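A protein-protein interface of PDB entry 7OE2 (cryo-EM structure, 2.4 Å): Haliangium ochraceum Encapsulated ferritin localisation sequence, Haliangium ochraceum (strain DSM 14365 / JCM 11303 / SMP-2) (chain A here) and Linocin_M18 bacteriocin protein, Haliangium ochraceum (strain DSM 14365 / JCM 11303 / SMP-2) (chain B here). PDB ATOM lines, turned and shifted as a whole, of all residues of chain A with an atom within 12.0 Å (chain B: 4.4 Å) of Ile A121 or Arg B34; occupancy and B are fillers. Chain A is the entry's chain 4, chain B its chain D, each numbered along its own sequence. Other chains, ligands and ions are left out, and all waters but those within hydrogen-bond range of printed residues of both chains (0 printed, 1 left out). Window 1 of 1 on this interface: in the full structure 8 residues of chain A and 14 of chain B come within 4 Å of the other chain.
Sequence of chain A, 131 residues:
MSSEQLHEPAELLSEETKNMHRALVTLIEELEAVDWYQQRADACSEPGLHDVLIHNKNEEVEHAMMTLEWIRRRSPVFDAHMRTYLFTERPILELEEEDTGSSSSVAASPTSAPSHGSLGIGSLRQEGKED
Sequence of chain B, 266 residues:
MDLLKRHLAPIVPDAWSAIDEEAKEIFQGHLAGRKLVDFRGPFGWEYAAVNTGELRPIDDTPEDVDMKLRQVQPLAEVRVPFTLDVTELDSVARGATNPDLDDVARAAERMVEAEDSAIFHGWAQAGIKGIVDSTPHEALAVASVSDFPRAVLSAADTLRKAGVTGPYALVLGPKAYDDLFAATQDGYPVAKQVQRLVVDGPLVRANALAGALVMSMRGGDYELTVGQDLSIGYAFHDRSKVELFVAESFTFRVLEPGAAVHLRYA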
ATOM      1  N   GLY A 117     -16.373  38.209 -20.822  1.00  0.00           N
ATOM      2  CA  GLY A 117     -15.736  39.089 -21.785  1.00  0.00           C
ATOM      3  C   GLY A 117     -14.765  38.384 -22.712  1.00  0.00           C
ATOM      4  O   GLY A 117     -13.714  38.916 -23.042  1.00  0.00           O
ATOM      5  N   SER A 118     -15.131  37.184 -23.146  1.00  0.00           N
ATOM      6  CA  SER A 118     -14.273  36.366 -23.982  1.00  0.00           C
ATOM      7  C   SER A 118     -14.519  36.660 -25.461  1.00  0.00           C
ATOM      8  O   SER A 118     -15.390  37.446 -25.835  1.00  0.00           O
ATOM      9  CB  SER A 118     -14.483  34.888 -23.657  1.00  0.00           C
ATOM     10  OG  SER A 118     -15.558  34.342 -24.393  1.00  0.00           O
ATOM     11  N   LEU A 119     -13.724  36.025 -26.318  1.00  0.00           N
ATOM     12  CA  LEU A 119     -13.884  36.162 -27.760  1.00  0.00           C
ATOM     13  C   LEU A 119     -15.105  35.430 -28.299  1.00  0.00           C
ATOM     14  O   LEU A 119     -15.468  35.646 -29.456  1.00  0.00           O
ATOM     15  CB  LEU A 119     -12.624  35.663 -28.466  1.00  0.00           C
ATOM     16  CG  LEU A 119     -11.401  36.549 -28.235  1.00  0.00           C
ATOM     17  CD1 LEU A 119     -10.114  35.798 -28.487  1.00  0.00           C
ATOM     18  CD2 LEU A 119     -11.490  37.786 -29.105  1.00  0.00           C
ATOM     19  N   GLY A 120     -15.743  34.584 -27.497  1.00  0.00           N
ATOM     20  CA  GLY A 120     -16.931  33.876 -27.931  1.00  0.00           C
ATOM     21  C   GLY A 120     -16.692  32.724 -28.882  1.00  0.00           C
ATOM     22  O   GLY A 120     -17.510  32.489 -29.775  1.00  0.00           O
ATOM     23  N   ILE A 121     -15.591  31.992 -28.715  1.00  0.00           N
ATOM     24  CA  ILE A 121     -15.302  30.870 -29.604  1.00  0.00           C
ATOM     25  C   ILE A 121     -16.213  29.691 -29.282  1.00  0.00           C
ATOM     26  O   ILE A 121     -16.992  29.238 -30.125  1.00  0.00           O
ATOM     27  CB  ILE A 121     -13.817  30.474 -29.516  1.00  0.00           C
ATOM     28  CG1 ILE A 121     -12.919  31.689 -29.765  1.00  0.00           C
ATOM     29  CG2 ILE A 121     -13.503  29.359 -30.500  1.00  0.00           C
ATOM     30  CD1 ILE A 121     -13.174  32.387 -31.077  1.00  0.00           C
ATOM     31  N   GLY A 122     -16.127  29.181 -28.057  1.00  0.00           N
ATOM     32  CA  GLY A 122     -16.948  28.061 -27.654  1.00  0.00           C
ATOM     33  C   GLY A 122     -16.623  26.784 -28.418  1.00  0.00           C
ATOM     34  O   GLY A 122     -15.529  26.591 -28.948  1.00  0.00           O
ATOM     35  N   SER A 123     -17.615  25.901 -28.462  1.00  0.00           N
ATOM     36  CA  SER A 123     -17.499  24.671 -29.232  1.00  0.00           C
ATOM     37  C   SER A 123     -17.436  24.979 -30.723  1.00  0.00           C
ATOM     38  O   SER A 123     -18.141  25.858 -31.223  1.00  0.00           O
ATOM     39  CB  SER A 123     -18.682  23.752 -28.941  1.00  0.00           C
ATOM     40  OG  SER A 123     -18.487  22.471 -29.508  1.00  0.00           O
ATOM     41  N   LEU A 124     -16.582  24.252 -31.437  1.00  0.00           N
ATOM     42  CA  LEU A 124     -16.442  24.443 -32.871  1.00  0.00           C
ATOM     43  C   LEU A 124     -17.069  23.331 -33.701  1.00  0.00           C
ATOM     44  O   LEU A 124     -17.168  23.483 -34.923  1.00  0.00           O
ATOM     45  CB  LEU A 124     -14.961  24.605 -33.245  1.00  0.00           C
ATOM     46  CG  LEU A 124     -14.399  25.989 -32.893  1.00  0.00           C
ATOM     47  CD1 LEU A 124     -13.006  26.210 -33.452  1.00  0.00           C
ATOM     48  CD2 LEU A 124     -15.341  27.083 -33.365  1.00  0.00           C
ATOM     49  N   ARG A 125     -17.497  22.234 -33.079  1.00  0.00           N
ATOM     50  CA  ARG A 125     -18.288  21.194 -33.741  1.00  0.00           C
ATOM     51  C   ARG A 125     -18.773  20.164 -32.728  1.00  0.00           C
ATOM     52  O   ARG A 125     -17.983  19.398 -32.179  1.00  0.00           O
ATOM     53  CB  ARG A 125     -17.491  20.511 -34.839  1.00  0.00           C
ATOM     54  N   LYS B  24     -10.022  36.101 -33.453  1.00  0.00           N
ATOM     55  CA  LYS B  24     -11.186  35.252 -33.659  1.00  0.00           C
ATOM     56  C   LYS B  24     -11.105  34.473 -34.962  1.00  0.00           C
ATOM     57  O   LYS B  24     -11.511  33.309 -35.007  1.00  0.00           O
ATOM     58  CB  LYS B  24     -12.445  36.110 -33.625  1.00  0.00           C
ATOM     59  CG  LYS B  24     -13.720  35.347 -33.422  1.00  0.00           C
ATOM     60  CD  LYS B  24     -14.817  36.240 -32.879  1.00  0.00           C
ATOM     61  CE  LYS B  24     -14.243  37.422 -32.104  1.00  0.00           C
ATOM     62  NZ  LYS B  24     -15.295  38.280 -31.499  1.00  0.00           N
ATOM     63  N   PHE B  27      -8.755  31.621 -34.364  1.00  0.00           N
ATOM     64  CA  PHE B  27      -9.304  30.594 -33.486  1.00  0.00           C
ATOM     65  C   PHE B  27     -10.369  29.767 -34.192  1.00  0.00           C
ATOM     66  O   PHE B  27     -10.371  28.538 -34.090  1.00  0.00           O
ATOM     67  CB  PHE B  27      -9.861  31.221 -32.210  1.00  0.00           C
ATOM     68  CG  PHE B  27      -8.805  31.711 -31.278  1.00  0.00           C
ATOM     69  CD1 PHE B  27      -7.651  30.983 -31.085  1.00  0.00           C
ATOM     70  CD2 PHE B  27      -8.953  32.908 -30.608  1.00  0.00           C
ATOM     71  CE1 PHE B  27      -6.676  31.432 -30.237  1.00  0.00           C
ATOM     72  CE2 PHE B  27      -7.975  33.358 -29.769  1.00  0.00           C
ATOM     73  CZ  PHE B  27      -6.841  32.624 -29.580  1.00  0.00           C
ATOM     74  N   LEU B  31      -8.593  25.835 -34.492  1.00  0.00           N
ATOM     75  CA  LEU B  31      -8.803  25.027 -33.288  1.00  0.00           C
ATOM     76  C   LEU B  31      -9.406  23.686 -33.689  1.00  0.00           C
ATOM     77  O   LEU B  31     -10.608  23.579 -33.929  1.00  0.00           O
ATOM     78  CB  LEU B  31      -9.697  25.756 -32.297  1.00  0.00           C
ATOM     79  CG  LEU B  31      -9.030  26.793 -31.396  1.00  0.00           C
ATOM     80  CD1 LEU B  31     -10.083  27.620 -30.712  1.00  0.00           C
ATOM     81  CD2 LEU B  31      -8.107  26.137 -30.393  1.00  0.00           C
ATOM     82  N   ALA B  32      -8.574  22.650 -33.742  1.00  0.00           N
ATOM     83  CA  ALA B  32      -9.031  21.359 -34.244  1.00  0.00           C
ATOM     84  C   ALA B  32      -9.661  20.505 -33.148  1.00  0.00           C
ATOM     85  O   ALA B  32     -10.666  19.834 -33.392  1.00  0.00           O
ATOM     86  CB  ALA B  32      -7.870  20.618 -34.901  1.00  0.00           C
ATOM     87  N   GLY B  33      -9.090  20.518 -31.943  1.00  0.00           N
ATOM     88  CA  GLY B  33      -9.634  19.709 -30.863  1.00  0.00           C
ATOM     89  C   GLY B  33     -11.074  20.049 -30.528  1.00  0.00           C
ATOM     90  O   GLY B  33     -11.880  19.162 -30.251  1.00  0.00           O
ATOM     91  N   ARG B  34     -11.420  21.336 -30.556  1.00  0.00           N
ATOM     92  CA  ARG B  34     -12.785  21.754 -30.259  1.00  0.00           C
ATOM     93  C   ARG B  34     -13.785  21.297 -31.309  1.00  0.00           C
ATOM     94  O   ARG B  34     -14.985  21.287 -31.036  1.00  0.00           O
ATOM     95  CB  ARG B  34     -12.845  23.270 -30.116  1.00  0.00           C
ATOM     96  CG  ARG B  34     -12.313  23.760 -28.806  1.00  0.00           C
ATOM     97  CD  ARG B  34     -11.848  25.172 -28.916  1.00  0.00           C
ATOM     98  NE  ARG B  34     -12.792  26.125 -28.368  1.00  0.00           N
ATOM     99  CZ  ARG B  34     -12.574  26.856 -27.287  1.00  0.00           C
ATOM    100  NH1 ARG B  34     -11.438  26.749 -26.626  1.00  0.00           N
ATOM    101  NH2 ARG B  34     -13.497  27.699 -26.878  1.00  0.00           N
ATOM    102  N   LYS B  35     -13.323  20.927 -32.500  1.00  0.00           N
ATOM    103  CA  LYS B  35     -14.209  20.355 -33.501  1.00  0.00           C
ATOM    104  C   LYS B  35     -14.551  18.899 -33.224  1.00  0.00           C
ATOM    105  O   LYS B  35     -15.540  18.401 -33.761  1.00  0.00           O
ATOM    106  CB  LYS B  35     -13.581  20.464 -34.891  1.00  0.00           C
ATOM    107  CG  LYS B  35     -13.700  21.821 -35.534  1.00  0.00           C
ATOM    108  CD  LYS B  35     -12.461  22.153 -36.335  1.00  0.00           C
ATOM    109  CE  LYS B  35     -12.654  23.426 -37.138  1.00  0.00           C
ATOM    110  NZ  LYS B  35     -11.416  24.251 -37.189  1.00  0.00           N
ATOM    111  N   LEU B  36     -13.773  18.208 -32.399  1.00  0.00           N
ATOM    112  CA  LEU B  36     -13.871  16.762 -32.288  1.00  0.00           C
ATOM    113  C   LEU B  36     -14.372  16.261 -30.946  1.00  0.00           C
ATOM    114  O   LEU B  36     -14.961  15.185 -30.895  1.00  0.00           O
ATOM    115  CB  LEU B  36     -12.507  16.127 -32.573  1.00  0.00           C
ATOM    116  CG  LEU B  36     -11.970  16.461 -33.963  1.00  0.00           C
ATOM    117  CD1 LEU B  36     -10.476  16.253 -34.047  1.00  0.00           C
ATOM    118  CD2 LEU B  36     -12.704  15.649 -35.018  1.00  0.00           C
ATOM    119  N   VAL B  37     -14.166  16.999 -29.865  1.00  0.00           N
ATOM    120  CA  VAL B  37     -14.436  16.496 -28.529  1.00  0.00           C
ATOM    121  C   VAL B  37     -15.686  17.170 -27.976  1.00  0.00           C
ATOM    122  O   VAL B  37     -16.171  18.170 -28.504  1.00  0.00           O
ATOM    123  CB  VAL B  37     -13.221  16.696 -27.595  1.00  0.00           C
ATOM    124  CG1 VAL B  37     -11.979  16.092 -28.219  1.00  0.00           C
ATOM    125  CG2 VAL B  37     -13.000  18.166 -27.293  1.00  0.00           C
ATOM    126  N   PHE B  39     -17.685  19.501 -25.504  1.00  0.00           N
ATOM    127  CA  PHE B  39     -17.342  20.810 -24.971  1.00  0.00           C
ATOM    128  C   PHE B  39     -18.205  21.092 -23.752  1.00  0.00           C
ATOM    129  O   PHE B  39     -19.427  21.203 -23.865  1.00  0.00           O
ATOM    130  CB  PHE B  39     -17.535  21.889 -26.034  1.00  0.00           C
ATOM    131  CG  PHE B  39     -16.931  23.212 -25.676  1.00  0.00           C
ATOM    132  CD1 PHE B  39     -15.615  23.493 -25.984  1.00  0.00           C
ATOM    133  CD2 PHE B  39     -17.683  24.182 -25.040  1.00  0.00           C
ATOM    134  CE1 PHE B  39     -15.063  24.706 -25.665  1.00  0.00           C
ATOM    135  CE2 PHE B  39     -17.131  25.396 -24.714  1.00  0.00           C
ATOM    136  CZ  PHE B  39     -15.821  25.659 -25.030  1.00  0.00           C
ATOM    137  N   GLU B 115      -3.483  24.517 -26.723  1.00  0.00           N
ATOM    138  CA  GLU B 115      -4.717  23.772 -26.485  1.00  0.00           C
ATOM    139  C   GLU B 115      -4.750  22.472 -27.284  1.00  0.00           C
ATOM    140  O   GLU B 115      -5.057  21.402 -26.741  1.00  0.00           O
ATOM    141  CB  GLU B 115      -5.937  24.633 -26.818  1.00  0.00           C
ATOM    142  CG  GLU B 115      -7.239  24.092 -26.232  1.00  0.00           C
ATOM    143  CD  GLU B 115      -8.484  24.465 -27.031  1.00  0.00           C
ATOM    144  OE1 GLU B 115      -9.082  25.523 -26.764  1.00  0.00           O
ATOM    145  OE2 GLU B 115      -8.881  23.688 -27.917  1.00  0.00           O
ATOM    146  N   LEU B 224     -13.479  18.365 -23.224  1.00  0.00           N
ATOM    147  CA  LEU B 224     -12.750  19.589 -22.946  1.00  0.00           C
ATOM    148  C   LEU B 224     -13.646  20.498 -22.120  1.00  0.00           C
ATOM    149  O   LEU B 224     -14.742  20.848 -22.553  1.00  0.00           O
ATOM    150  CB  LEU B 224     -12.332  20.272 -24.246  1.00  0.00           C
ATOM    151  CG  LEU B 224     -11.626  21.620 -24.145  1.00  0.00           C
ATOM    152  CD1 LEU B 224     -10.182  21.434 -23.720  1.00  0.00           C
ATOM    153  CD2 LEU B 224     -11.722  22.360 -25.459  1.00  0.00           C
ATOM    154  N   VAL B 226     -14.038  24.175 -20.406  1.00  0.00           N
ATOM    155  CA  VAL B 226     -13.525  25.533 -20.445  1.00  0.00           C
ATOM    156  C   VAL B 226     -14.103  26.310 -19.274  1.00  0.00           C
ATOM    157  O   VAL B 226     -15.300  26.231 -18.986  1.00  0.00           O
ATOM    158  CB  VAL B 226     -13.835  26.213 -21.794  1.00  0.00           C
ATOM    159  CG1 VAL B 226     -13.647  27.702 -21.705  1.00  0.00           C
ATOM    160  CG2 VAL B 226     -12.947  25.640 -22.876  1.00  0.00           C
ATOM    161  N   ASP B 229     -13.176  31.313 -21.321  1.00  0.00           N
ATOM    162  CA  ASP B 229     -12.913  31.045 -22.723  1.00  0.00           C
ATOM    163  C   ASP B 229     -11.875  32.024 -23.265  1.00  0.00           C
ATOM    164  O   ASP B 229     -11.537  33.022 -22.630  1.00  0.00           O
ATOM    165  CB  ASP B 229     -14.201  31.113 -23.535  1.00  0.00           C
ATOM    166  CG  ASP B 229     -14.186  30.184 -24.736  1.00  0.00           C
ATOM    167  OD1 ASP B 229     -13.168  29.509 -24.967  1.00  0.00           O
ATOM    168  OD2 ASP B 229     -15.198  30.127 -25.453  1.00  0.00           O
ATOM    169  N   LEU B 230     -11.363  31.707 -24.452  1.00  0.00           N
ATOM    170  CA  LEU B 230     -10.345  32.504 -25.129  1.00  0.00           C
ATOM    171  C   LEU B 230     -10.688  33.986 -25.123  1.00  0.00           C
ATOM    172  O   LEU B 230     -11.739  34.394 -25.613  1.00  0.00           O
ATOM    173  CB  LEU B 230     -10.180  32.004 -26.563  1.00  0.00           C
ATOM    174  CG  LEU B 230      -9.549  30.620 -26.693  1.00  0.00           C
ATOM    175  CD1 LEU B 230      -9.839  30.005 -28.044  1.00  0.00           C
ATOM    176  CD2 LEU B 230      -8.071  30.703 -26.448  1.00  0.00           C
ATOM    177  N   GLU B 248      -6.903  31.843 -21.408  1.00  0.00           N
ATOM    178  CA  GLU B 248      -7.901  30.783 -21.375  1.00  0.00           C
ATOM    179  C   GLU B 248      -7.673  29.923 -20.142  1.00  0.00           C
ATOM    180  O   GLU B 248      -6.540  29.703 -19.731  1.00  0.00           O
ATOM    181  CB  GLU B 248      -7.856  29.909 -22.638  1.00  0.00           C
ATOM    182  CG  GLU B 248      -9.144  29.159 -22.885  1.00  0.00           C
ATOM    183  CD  GLU B 248      -9.027  28.063 -23.922  1.00  0.00           C
ATOM    184  OE1 GLU B 248     -10.048  27.766 -24.572  1.00  0.00           O
ATOM    185  OE2 GLU B 248      -7.927  27.501 -24.099  1.00  0.00           O
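N of Arg A125 lies within hydrogen-bond range of O of Arg B34 (3.4 Å).
The guanidinium group of Arg B34 sits at hydrogen-bond distance from the backbone carbonyl oxygen of Gly A122 (2.8 Å).
O of Lys B35 sits close to O of Arg A125.
The side-chain amino group of Lys B24 sits at hydrogen-bond distance from the backbone carbonyl oxygen of Leu A119.
O of Leu B230 is in hydrogen-bond range of N of Leu A119, at 2.7 Å.
The backbone NH (N) of Leu A124 sits at hydrogen-bond distance from the backbone carbonyl oxygen (O) of Arg B34 (3.4 Å).
The backbone NH (N) of Gly A122 is in hydrogen-bond range of the side-chain carboxylate (OD2) of Asp B229.
The guanidinium group of Arg B34 lies within salt-bridge range of the side-chain carboxylate of Glu B115 (2.7 Å).
The guanidinium group (NH2) of Arg B34 lies within salt-bridge range of the side-chain carboxylate (OD1) of Asp B229, 2.7 Å away.
OE1 of Glu B248 is in salt-bridge range of NH1 of Arg B34.
The backbone NH of Gly A120 sits at hydrogen-bond distance from the side-chain hydroxyl of Ser A118 (3.1 Å).
O of Leu B31 lies close to NZ of Lys B35 (3.4 Å).
Among the printed residues, pairs that only touch across the chains: Ser A118 with Asp B229 (3.6 Å), Ser A118 with Leu B230 (3.4 Å), Leu A119 with Phe B27 (3.5 Å), Ile A121 with Lys B24 (3.8 Å), Ile A121 with Phe B27 (3.7 Å), Ile A121 with Leu B31 (3.8 Å), Ile A121 with Arg B34 (3.8 Å), Ile A121 with Asp B229 (3.8 Å), Ile A121 with Leu B230 (3.9 Å), Gly A122 with Phe B39 (3.7 Å), Ser A123 with Phe B39 (3.6 Å), Leu A124 with Phe B27 (3.6 Å), Leu A124 with Leu B31 (3.5 Å) and Leu A124 with Lys B35 (3.8 Å).
Printed residues of chain B within 4 Å of Ser A118: Asp B229 (3.6 Å) and Leu B230 (3.4 Å).
Of chain A, only Leu A119 and Ile A121 come within 4 Å of Lys B24.
Phe B27 touches three residues of chain A.
Leu B31 touches just these residues of chain A: Ile A121 and Leu A124.
Ala B32 touches none of the printed residues of chain A.
No residue of chain A comes within 4 Å of Gly B33.
Of the printed residues of chain A, Arg B34 touches Ile A121 (3.8 Å), Gly A122 (2.8 Å), Leu A124 (3.4 Å) and Arg A125 (3.4 Å).
Lys B35 touches two residues of chain A.
No residue of chain A comes within 4 Å of Leu B36.
No residue of chain A comes within 4 Å of Val B37.
Of the printed residues of chain A, Phe B39 touches Gly A122 (3.7 Å) and Ser A123 (3.6 Å).
No residue of chain A comes within 4 Å of Leu B224.
Asp B229 touches just these residues of chain A: Ser A118, Ile A121 and Gly A122.
Of chain A, only Ser A118, Leu A119 and Ile A121 come within 4 Å of Leu B230.
The nearest printed residue of chain B that does not touch Leu A119 is Asp B229 (5.2 Å).
Of the 16 printed residues of chain B, 8 touch a printed residue of chain A.
Printed residues of chain B that touch a printed residue of chain A: Lys B24, Phe B27, Leu B31, Arg B34, Lys B35, Phe B39, Asp B229 and Leu B230.
Along chain B the printed residues that touch a printed residue of chain A span positions 24 to 230.
Of the 9 printed residues of chain A, 7 touch a printed residue of chain B.
Hydrophobic or aromatic side chains of chain A within 4 Å of the printed part of chain B: Leu A119, Ile A121 and Leu A124.
Among the printed residues, no Asp or Glu carboxylate lies within 4 Å of a Lys or Arg side-chain nitrogen of the other chain.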
